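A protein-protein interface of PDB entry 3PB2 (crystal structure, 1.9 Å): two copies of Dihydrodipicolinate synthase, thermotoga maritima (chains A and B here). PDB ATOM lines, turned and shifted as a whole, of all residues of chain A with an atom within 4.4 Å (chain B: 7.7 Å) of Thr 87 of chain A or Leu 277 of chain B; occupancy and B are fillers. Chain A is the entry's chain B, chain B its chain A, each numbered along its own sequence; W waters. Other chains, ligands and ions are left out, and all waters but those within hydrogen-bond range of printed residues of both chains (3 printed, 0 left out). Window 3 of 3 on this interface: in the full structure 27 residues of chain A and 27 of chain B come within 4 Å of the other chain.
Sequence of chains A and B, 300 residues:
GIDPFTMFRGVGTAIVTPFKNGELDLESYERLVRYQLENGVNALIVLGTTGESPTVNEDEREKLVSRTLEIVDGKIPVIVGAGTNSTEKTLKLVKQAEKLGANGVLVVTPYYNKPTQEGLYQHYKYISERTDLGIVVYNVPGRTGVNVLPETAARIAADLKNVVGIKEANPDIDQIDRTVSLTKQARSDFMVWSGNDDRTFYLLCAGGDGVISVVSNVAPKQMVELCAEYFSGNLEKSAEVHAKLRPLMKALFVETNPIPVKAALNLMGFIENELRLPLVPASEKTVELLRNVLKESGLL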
ATOM      1  N   ASN A  85     -26.899  32.395  26.948  1.00  0.00           N
ATOM      2  CA  ASN A  85     -26.077  31.296  27.428  1.00  0.00           C
ATOM      3  C   ASN A  85     -24.966  30.912  26.435  1.00  0.00           C
ATOM      4  O   ASN A  85     -24.288  29.898  26.610  1.00  0.00           O
ATOM      5  CB  ASN A  85     -26.943  30.097  27.847  1.00  0.00           C
ATOM      6  CG  ASN A  85     -27.757  29.509  26.686  1.00  0.00           C
ATOM      7  OD1 ASN A  85     -27.728  30.017  25.564  1.00  0.00           O
ATOM      8  ND2 ASN A  85     -28.489  28.436  26.964  1.00  0.00           N
ATOM      9  N   SER A  86     -24.797  31.734  25.398  1.00  0.00           N
ATOM     10  CA  SER A  86     -23.682  31.589  24.462  1.00  0.00           C
ATOM     11  C   SER A  86     -22.728  32.746  24.623  1.00  0.00           C
ATOM     12  O   SER A  86     -23.141  33.898  24.494  1.00  0.00           O
ATOM     13  CB  SER A  86     -24.184  31.560  23.007  1.00  0.00           C
ATOM     14  OG  SER A  86     -23.110  31.853  22.124  1.00  0.00           O
ATOM     15  N   THR A  87     -21.460  32.465  24.910  1.00  0.00           N
ATOM     16  CA  THR A  87     -20.491  33.555  25.118  1.00  0.00           C
ATOM     17  C   THR A  87     -20.338  34.444  23.873  1.00  0.00           C
ATOM     18  O   THR A  87     -20.292  35.667  23.974  1.00  0.00           O
ATOM     19  CB  THR A  87     -19.114  33.026  25.569  1.00  0.00           C
ATOM     20  OG1 THR A  87     -19.267  32.277  26.785  1.00  0.00           O
ATOM     21  CG2 THR A  87     -18.132  34.185  25.814  1.00  0.00           C
ATOM     22  N   GLU A  88     -20.255  33.818  22.708  1.00  0.00           N
ATOM     23  CA  GLU A  88     -20.164  34.543  21.448  1.00  0.00           C
ATOM     24  C   GLU A  88     -21.386  35.435  21.203  1.00  0.00           C
ATOM     25  O   GLU A  88     -21.247  36.608  20.875  1.00  0.00           O
ATOM     26  CB  GLU A  88     -19.998  33.567  20.280  1.00  0.00           C
ATOM     27  CG  GLU A  88     -19.949  34.241  18.919  1.00  0.00           C
ATOM     28  CD  GLU A  88     -19.989  33.249  17.769  1.00  0.00           C
ATOM     29  OE1 GLU A  88     -19.579  32.084  17.965  1.00  0.00           O
ATOM     30  OE2 GLU A  88     -20.438  33.631  16.667  1.00  0.00           O
ATOM     31  N   LYS A  89     -22.582  34.882  21.350  1.00  0.00           N
ATOM     32  CA  LYS A  89     -23.796  35.660  21.096  1.00  0.00           C
ATOM     33  C   LYS A  89     -23.941  36.802  22.120  1.00  0.00           C
ATOM     34  O   LYS A  89     -24.396  37.897  21.791  1.00  0.00           O
ATOM     35  CB  LYS A  89     -25.033  34.758  21.101  1.00  0.00           C
ATOM     36  CG  LYS A  89     -26.358  35.512  21.010  1.00  0.00           C
ATOM     37  CD  LYS A  89     -26.354  36.463  19.813  1.00  0.00           C
ATOM     38  CE  LYS A  89     -27.610  37.331  19.744  1.00  0.00           C
ATOM     39  NZ  LYS A  89     -28.799  36.589  19.229  1.00  0.00           N
ATOM     40  N   THR A  90     -23.526  36.545  23.354  1.00  0.00           N
ATOM     41  CA  THR A  90     -23.602  37.560  24.402  1.00  0.00           C
ATOM     42  C   THR A  90     -22.751  38.770  24.023  1.00  0.00           C
ATOM     43  O   THR A  90     -23.169  39.927  24.184  1.00  0.00           O
ATOM     44  CB  THR A  90     -23.137  37.002  25.782  1.00  0.00           C
ATOM     45  OG1 THR A  90     -24.067  36.011  26.249  1.00  0.00           O
ATOM     46  CG2 THR A  90     -23.031  38.134  26.823  1.00  0.00           C
ATOM     47  N   LEU A  91     -21.556  38.522  23.499  1.00  0.00           N
ATOM     48  CA  LEU A  91     -20.721  39.644  23.086  1.00  0.00           C
ATOM     49  C   LEU A  91     -21.447  40.481  22.027  1.00  0.00           C
ATOM     50  O   LEU A  91     -21.457  41.715  22.089  1.00  0.00           O
ATOM     51  CB  LEU A  91     -19.356  39.174  22.571  1.00  0.00           C
ATOM     52  CG  LEU A  91     -18.437  40.295  22.056  1.00  0.00           C
ATOM     53  CD1 LEU A  91     -18.230  41.354  23.126  1.00  0.00           C
ATOM     54  CD2 LEU A  91     -17.095  39.728  21.590  1.00  0.00           C
ATOM     55  N   GLN A 122     -14.486  32.681  32.638  1.00  0.00           N
ATOM     56  CA  GLN A 122     -14.027  32.868  31.264  1.00  0.00           C
ATOM     57  C   GLN A 122     -15.062  33.587  30.401  1.00  0.00           C
ATOM     58  O   GLN A 122     -14.705  34.362  29.510  1.00  0.00           O
ATOM     59  CB  GLN A 122     -13.635  31.525  30.634  1.00  0.00           C
ATOM     60  CG  GLN A 122     -12.378  30.919  31.252  1.00  0.00           C
ATOM     61  CD  GLN A 122     -11.152  31.810  31.092  1.00  0.00           C
ATOM     62  OE1 GLN A 122     -11.046  32.581  30.133  1.00  0.00           O
ATOM     63  NE2 GLN A 122     -10.220  31.710  32.041  1.00  0.00           N
ATOM     64  N   HIS A 123     -16.340  33.322  30.674  1.00  0.00           N
ATOM     65  CA  HIS A 123     -17.449  33.996  29.990  1.00  0.00           C
ATOM     66  C   HIS A 123     -17.381  35.502  30.234  1.00  0.00           C
ATOM     67  O   HIS A 123     -17.369  36.284  29.276  1.00  0.00           O
ATOM     68  CB  HIS A 123     -18.785  33.402  30.473  1.00  0.00           C
ATOM     69  CG  HIS A 123     -20.011  34.080  29.933  1.00  0.00           C
ATOM     70  ND1 HIS A 123     -20.486  33.866  28.656  1.00  0.00           N
ATOM     71  CD2 HIS A 123     -20.896  34.917  30.524  1.00  0.00           C
ATOM     72  CE1 HIS A 123     -21.596  34.562  28.476  1.00  0.00           C
ATOM     73  NE2 HIS A 123     -21.871  35.206  29.597  1.00  0.00           N
ATOM     74  N   TYR A 126     -14.125  37.046  28.739  1.00  0.00           N
ATOM     75  CA  TYR A 126     -14.179  37.201  27.289  1.00  0.00           C
ATOM     76  C   TYR A 126     -14.933  38.472  26.906  1.00  0.00           C
ATOM     77  O   TYR A 126     -14.494  39.234  26.053  1.00  0.00           O
ATOM     78  CB  TYR A 126     -14.834  35.984  26.628  1.00  0.00           C
ATOM     79  CG  TYR A 126     -14.816  36.060  25.119  1.00  0.00           C
ATOM     80  CD1 TYR A 126     -13.671  35.714  24.401  1.00  0.00           C
ATOM     81  CD2 TYR A 126     -15.928  36.491  24.414  1.00  0.00           C
ATOM     82  CE1 TYR A 126     -13.642  35.784  23.018  1.00  0.00           C
ATOM     83  CE2 TYR A 126     -15.907  36.573  23.020  1.00  0.00           C
ATOM     84  CZ  TYR A 126     -14.759  36.225  22.334  1.00  0.00           C
ATOM     85  OH  TYR A 126     -14.727  36.295  20.957  1.00  0.00           O
ATOM     86  N   PHE B  19     -16.329  19.578  17.562  1.00  0.00           N
ATOM     87  CA  PHE B  19     -15.716  20.783  17.030  1.00  0.00           C
ATOM     88  C   PHE B  19     -14.226  20.562  16.763  1.00  0.00           C
ATOM     89  O   PHE B  19     -13.563  19.742  17.422  1.00  0.00           O
ATOM     90  CB  PHE B  19     -15.877  21.937  18.027  1.00  0.00           C
ATOM     91  CG  PHE B  19     -17.310  22.254  18.381  1.00  0.00           C
ATOM     92  CD1 PHE B  19     -18.262  22.445  17.388  1.00  0.00           C
ATOM     93  CD2 PHE B  19     -17.702  22.361  19.713  1.00  0.00           C
ATOM     94  CE1 PHE B  19     -19.580  22.753  17.714  1.00  0.00           C
ATOM     95  CE2 PHE B  19     -19.023  22.665  20.052  1.00  0.00           C
ATOM     96  CZ  PHE B  19     -19.957  22.858  19.057  1.00  0.00           C
ATOM     97  N   GLU B  52     -24.619  20.564  22.616  1.00  0.00           N
ATOM     98  CA  GLU B  52     -24.286  21.989  22.756  1.00  0.00           C
ATOM     99  C   GLU B  52     -25.122  22.922  21.886  1.00  0.00           C
ATOM    100  O   GLU B  52     -24.604  23.857  21.277  1.00  0.00           O
ATOM    101  CB  GLU B  52     -22.786  22.224  22.540  1.00  0.00           C
ATOM    102  CG  GLU B  52     -21.916  21.724  23.714  1.00  0.00           C
ATOM    103  CD  GLU B  52     -20.436  21.734  23.365  1.00  0.00           C
ATOM    104  OE1 GLU B  52     -19.803  22.806  23.489  1.00  0.00           O
ATOM    105  OE2 GLU B  52     -19.912  20.683  22.942  1.00  0.00           O
ATOM    106  N   PRO B  54     -26.873  25.411  22.562  1.00  0.00           N
ATOM    107  CA  PRO B  54     -26.790  26.854  22.814  1.00  0.00           C
ATOM    108  C   PRO B  54     -25.701  27.581  22.030  1.00  0.00           C
ATOM    109  O   PRO B  54     -25.813  28.796  21.811  1.00  0.00           O
ATOM    110  CB  PRO B  54     -26.509  26.937  24.329  1.00  0.00           C
ATOM    111  CG  PRO B  54     -27.070  25.646  24.880  1.00  0.00           C
ATOM    112  CD  PRO B  54     -26.818  24.617  23.805  1.00  0.00           C
ATOM    113  N   THR B  55     -24.667  26.869  21.600  1.00  0.00           N
ATOM    114  CA  THR B  55     -23.541  27.537  20.956  1.00  0.00           C
ATOM    115  C   THR B  55     -23.329  27.143  19.495  1.00  0.00           C
ATOM    116  O   THR B  55     -22.290  27.456  18.926  1.00  0.00           O
ATOM    117  CB  THR B  55     -22.228  27.271  21.730  1.00  0.00           C
ATOM    118  OG1 THR B  55     -22.073  25.858  21.926  1.00  0.00           O
ATOM    119  CG2 THR B  55     -22.265  27.948  23.092  1.00  0.00           C
ATOM    120  N   LEU B 275     -14.831  22.361  23.228  1.00  0.00           N
ATOM    121  CA  LEU B 275     -16.186  22.785  23.552  1.00  0.00           C
ATOM    122  C   LEU B 275     -16.250  24.284  23.322  1.00  0.00           C
ATOM    123  O   LEU B 275     -15.218  24.923  23.110  1.00  0.00           O
ATOM    124  CB  LEU B 275     -16.494  22.481  25.016  1.00  0.00           C
ATOM    125  CG  LEU B 275     -16.518  20.992  25.370  1.00  0.00           C
ATOM    126  CD1 LEU B 275     -15.210  20.552  26.043  1.00  0.00           C
ATOM    127  CD2 LEU B 275     -17.746  20.724  26.242  1.00  0.00           C
ATOM    128  N   ARG B 276     -17.441  24.863  23.396  1.00  0.00           N
ATOM    129  CA  ARG B 276     -17.553  26.309  23.202  1.00  0.00           C
ATOM    130  C   ARG B 276     -17.965  27.036  24.490  1.00  0.00           C
ATOM    131  O   ARG B 276     -18.827  26.557  25.233  1.00  0.00           O
ATOM    132  CB  ARG B 276     -18.550  26.592  22.066  1.00  0.00           C
ATOM    133  CG  ARG B 276     -17.969  26.278  20.670  1.00  0.00           C
ATOM    134  CD  ARG B 276     -19.016  26.455  19.555  1.00  0.00           C
ATOM    135  NE  ARG B 276     -18.424  26.215  18.237  1.00  0.00           N
ATOM    136  CZ  ARG B 276     -19.117  26.210  17.102  1.00  0.00           C
ATOM    137  NH1 ARG B 276     -20.434  26.414  17.121  1.00  0.00           N
ATOM    138  NH2 ARG B 276     -18.497  25.991  15.951  1.00  0.00           N
ATOM    139  N   LEU B 277     -17.353  28.188  24.749  1.00  0.00           N
ATOM    140  CA  LEU B 277     -17.661  28.949  25.963  1.00  0.00           C
ATOM    141  C   LEU B 277     -19.165  29.205  25.994  1.00  0.00           C
ATOM    142  O   LEU B 277     -19.771  29.451  24.949  1.00  0.00           O
ATOM    143  CB  LEU B 277     -16.877  30.272  25.995  1.00  0.00           C
ATOM    144  CG  LEU B 277     -15.368  30.194  26.307  1.00  0.00           C
ATOM    145  CD1 LEU B 277     -14.723  31.581  26.223  1.00  0.00           C
ATOM    146  CD2 LEU B 277     -15.070  29.541  27.674  1.00  0.00           C
ATOM    147  N   PRO B 278     -19.774  29.163  27.193  1.00  0.00           N
ATOM    148  CA  PRO B 278     -19.111  29.087  28.502  1.00  0.00           C
ATOM    149  C   PRO B 278     -18.661  27.678  28.954  1.00  0.00           C
ATOM    150  O   PRO B 278     -18.217  27.536  30.093  1.00  0.00           O
ATOM    151  CB  PRO B 278     -20.178  29.671  29.454  1.00  0.00           C
ATOM    152  CG  PRO B 278     -21.475  29.196  28.843  1.00  0.00           C
ATOM    153  CD  PRO B 278     -21.244  29.254  27.329  1.00  0.00           C
ATOM    154  N   LEU B 279     -18.750  26.663  28.096  1.00  0.00           N
ATOM    155  CA  LEU B 279     -18.241  25.344  28.473  1.00  0.00           C
ATOM    156  C   LEU B 279     -16.730  25.299  28.220  1.00  0.00           C
ATOM    157  O   LEU B 279     -16.221  25.992  27.335  1.00  0.00           O
ATOM    158  CB  LEU B 279     -18.947  24.208  27.722  1.00  0.00           C
ATOM    159  CG  LEU B 279     -20.455  24.066  27.968  1.00  0.00           C
ATOM    160  CD1 LEU B 279     -20.967  22.774  27.353  1.00  0.00           C
ATOM    161  CD2 LEU B 279     -20.773  24.139  29.475  1.00  0.00           C
ATOM    162  N   VAL B 280     -16.019  24.518  29.023  1.00  0.00           N
ATOM    163  CA  VAL B 280     -14.558  24.421  28.909  1.00  0.00           C
ATOM    164  C   VAL B 280     -14.185  22.963  29.135  1.00  0.00           C
ATOM    165  O   VAL B 280     -14.973  22.206  29.711  1.00  0.00           O
ATOM    166  CB  VAL B 280     -13.783  25.297  29.958  1.00  0.00           C
ATOM    167  CG1 VAL B 280     -14.084  26.796  29.799  1.00  0.00           C
ATOM    168  CG2 VAL B 280     -14.074  24.829  31.390  1.00  0.00           C
ATOM    169  N   PRO B 281     -12.990  22.562  28.673  1.00  0.00           N
ATOM    170  CA  PRO B 281     -12.552  21.166  28.793  1.00  0.00           C
ATOM    171  C   PRO B 281     -12.532  20.655  30.237  1.00  0.00           C
ATOM    172  O   PRO B 281     -12.321  21.438  31.185  1.00  0.00           O
ATOM    173  CB  PRO B 281     -11.121  21.199  28.217  1.00  0.00           C
ATOM    174  CG  PRO B 281     -11.141  22.321  27.253  1.00  0.00           C
ATOM    175  CD  PRO B 281     -12.027  23.376  27.906  1.00  0.00           C
HETATM  176  O   HOH W   1     -27.813  30.212  22.852  1.00  0.00           O
HETATM  177  O   HOH W   2     -19.440  30.866  22.599  1.00  0.00           O
HETATM  178  O   HOH W   3     -20.743  29.830  19.814  1.00  0.00           O
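N of Lys 89 of chain A sits at hydrogen-bond distance from OG of Ser 86 of chain A, at 3.2 Å.
The side-chain hydroxyl of Thr 90 of chain A lies within hydrogen-bond range of the backbone carbonyl oxygen of Ser 86 of chain A (2.9 Å).
OG1 of Thr 87 of chain A lies within hydrogen-bond range of ND1 of His 123 of chain A (2.7 Å).
Thr 87 of chain A touches just these residues of chain B: Leu 277 and Pro 278.
Leu 277 of chain B touches two residues of chain A.
Of chain B, only Pro 54 (3.4 Å) comes within 4 Å of Ser 86 of chain A.
Of the printed residues of chain A, Pro 54 of chain B touches Asn 85 and Ser 86.
Printed residues of chain B within 4 Å of Gln 122 of chain A: Leu 277.
Of the printed residues of chain A, Pro 278 of chain B touches Asn 85 (3.2 Å) and Thr 87 (3.2 Å).
Of the printed residues of chain B, Asn 85 of chain A touches Pro 54 (3.5 Å) and Pro 278 (3.2 Å).
The nearest printed residue of chain A that does not touch Leu 277 of chain B is Tyr 126 of chain A (4.4 Å).
The nearest printed residue of chain A that does not touch Pro 54 of chain B is Lys 89 of chain A (6.1 Å).
Water W1 lies within hydrogen-bond range of O of Pro 54 of chain B (2.7 Å) and OD1 of Asn 85 of chain A (2.7 Å).
Water W2 lies within hydrogen-bond range of the backbone carbonyl oxygen (O) of Leu 277 of chain B, the backbone NH (N) of Glu 88 of chain A and the backbone NH (N) of Thr 87 of chain A.
Water W3 lies within hydrogen-bond range of the backbone carbonyl oxygen (O) of Thr 55 of chain B (3.0 Å) and the side-chain carboxylate (OE1) of Glu 88 of chain A (3.1 Å).
Asn 85 of chain A touches Pro 54 of chain B.
CD of Pro 278 of chain B touches O of Asn 85 of chain A (3.2 Å).
CB of Ser 86 of chain A touches O of Pro 54 of chain B (3.4 Å).
CD2 of Leu 277 of chain B touches CB of Gln 122 of chain A, 3.8 Å away.
The backbone carbonyl oxygen of Leu 277 of chain B lies close to the side-chain hydroxyl of Thr 87 of chain A, at 3.4 Å.
The side-chain hydroxyl (OG1) of Thr 87 of chain A sits close to the backbone nitrogen (N) of Pro 278 of chain B, 3.2 Å away.
Hydrophobic or aromatic side chains of chain B within 4 Å of the printed part of chain A: Pro 54, Leu 277 and Pro 278.
Of the 10 printed residues of chain A, 4 touch a printed residue of chain B.
No position is printed for both chains.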
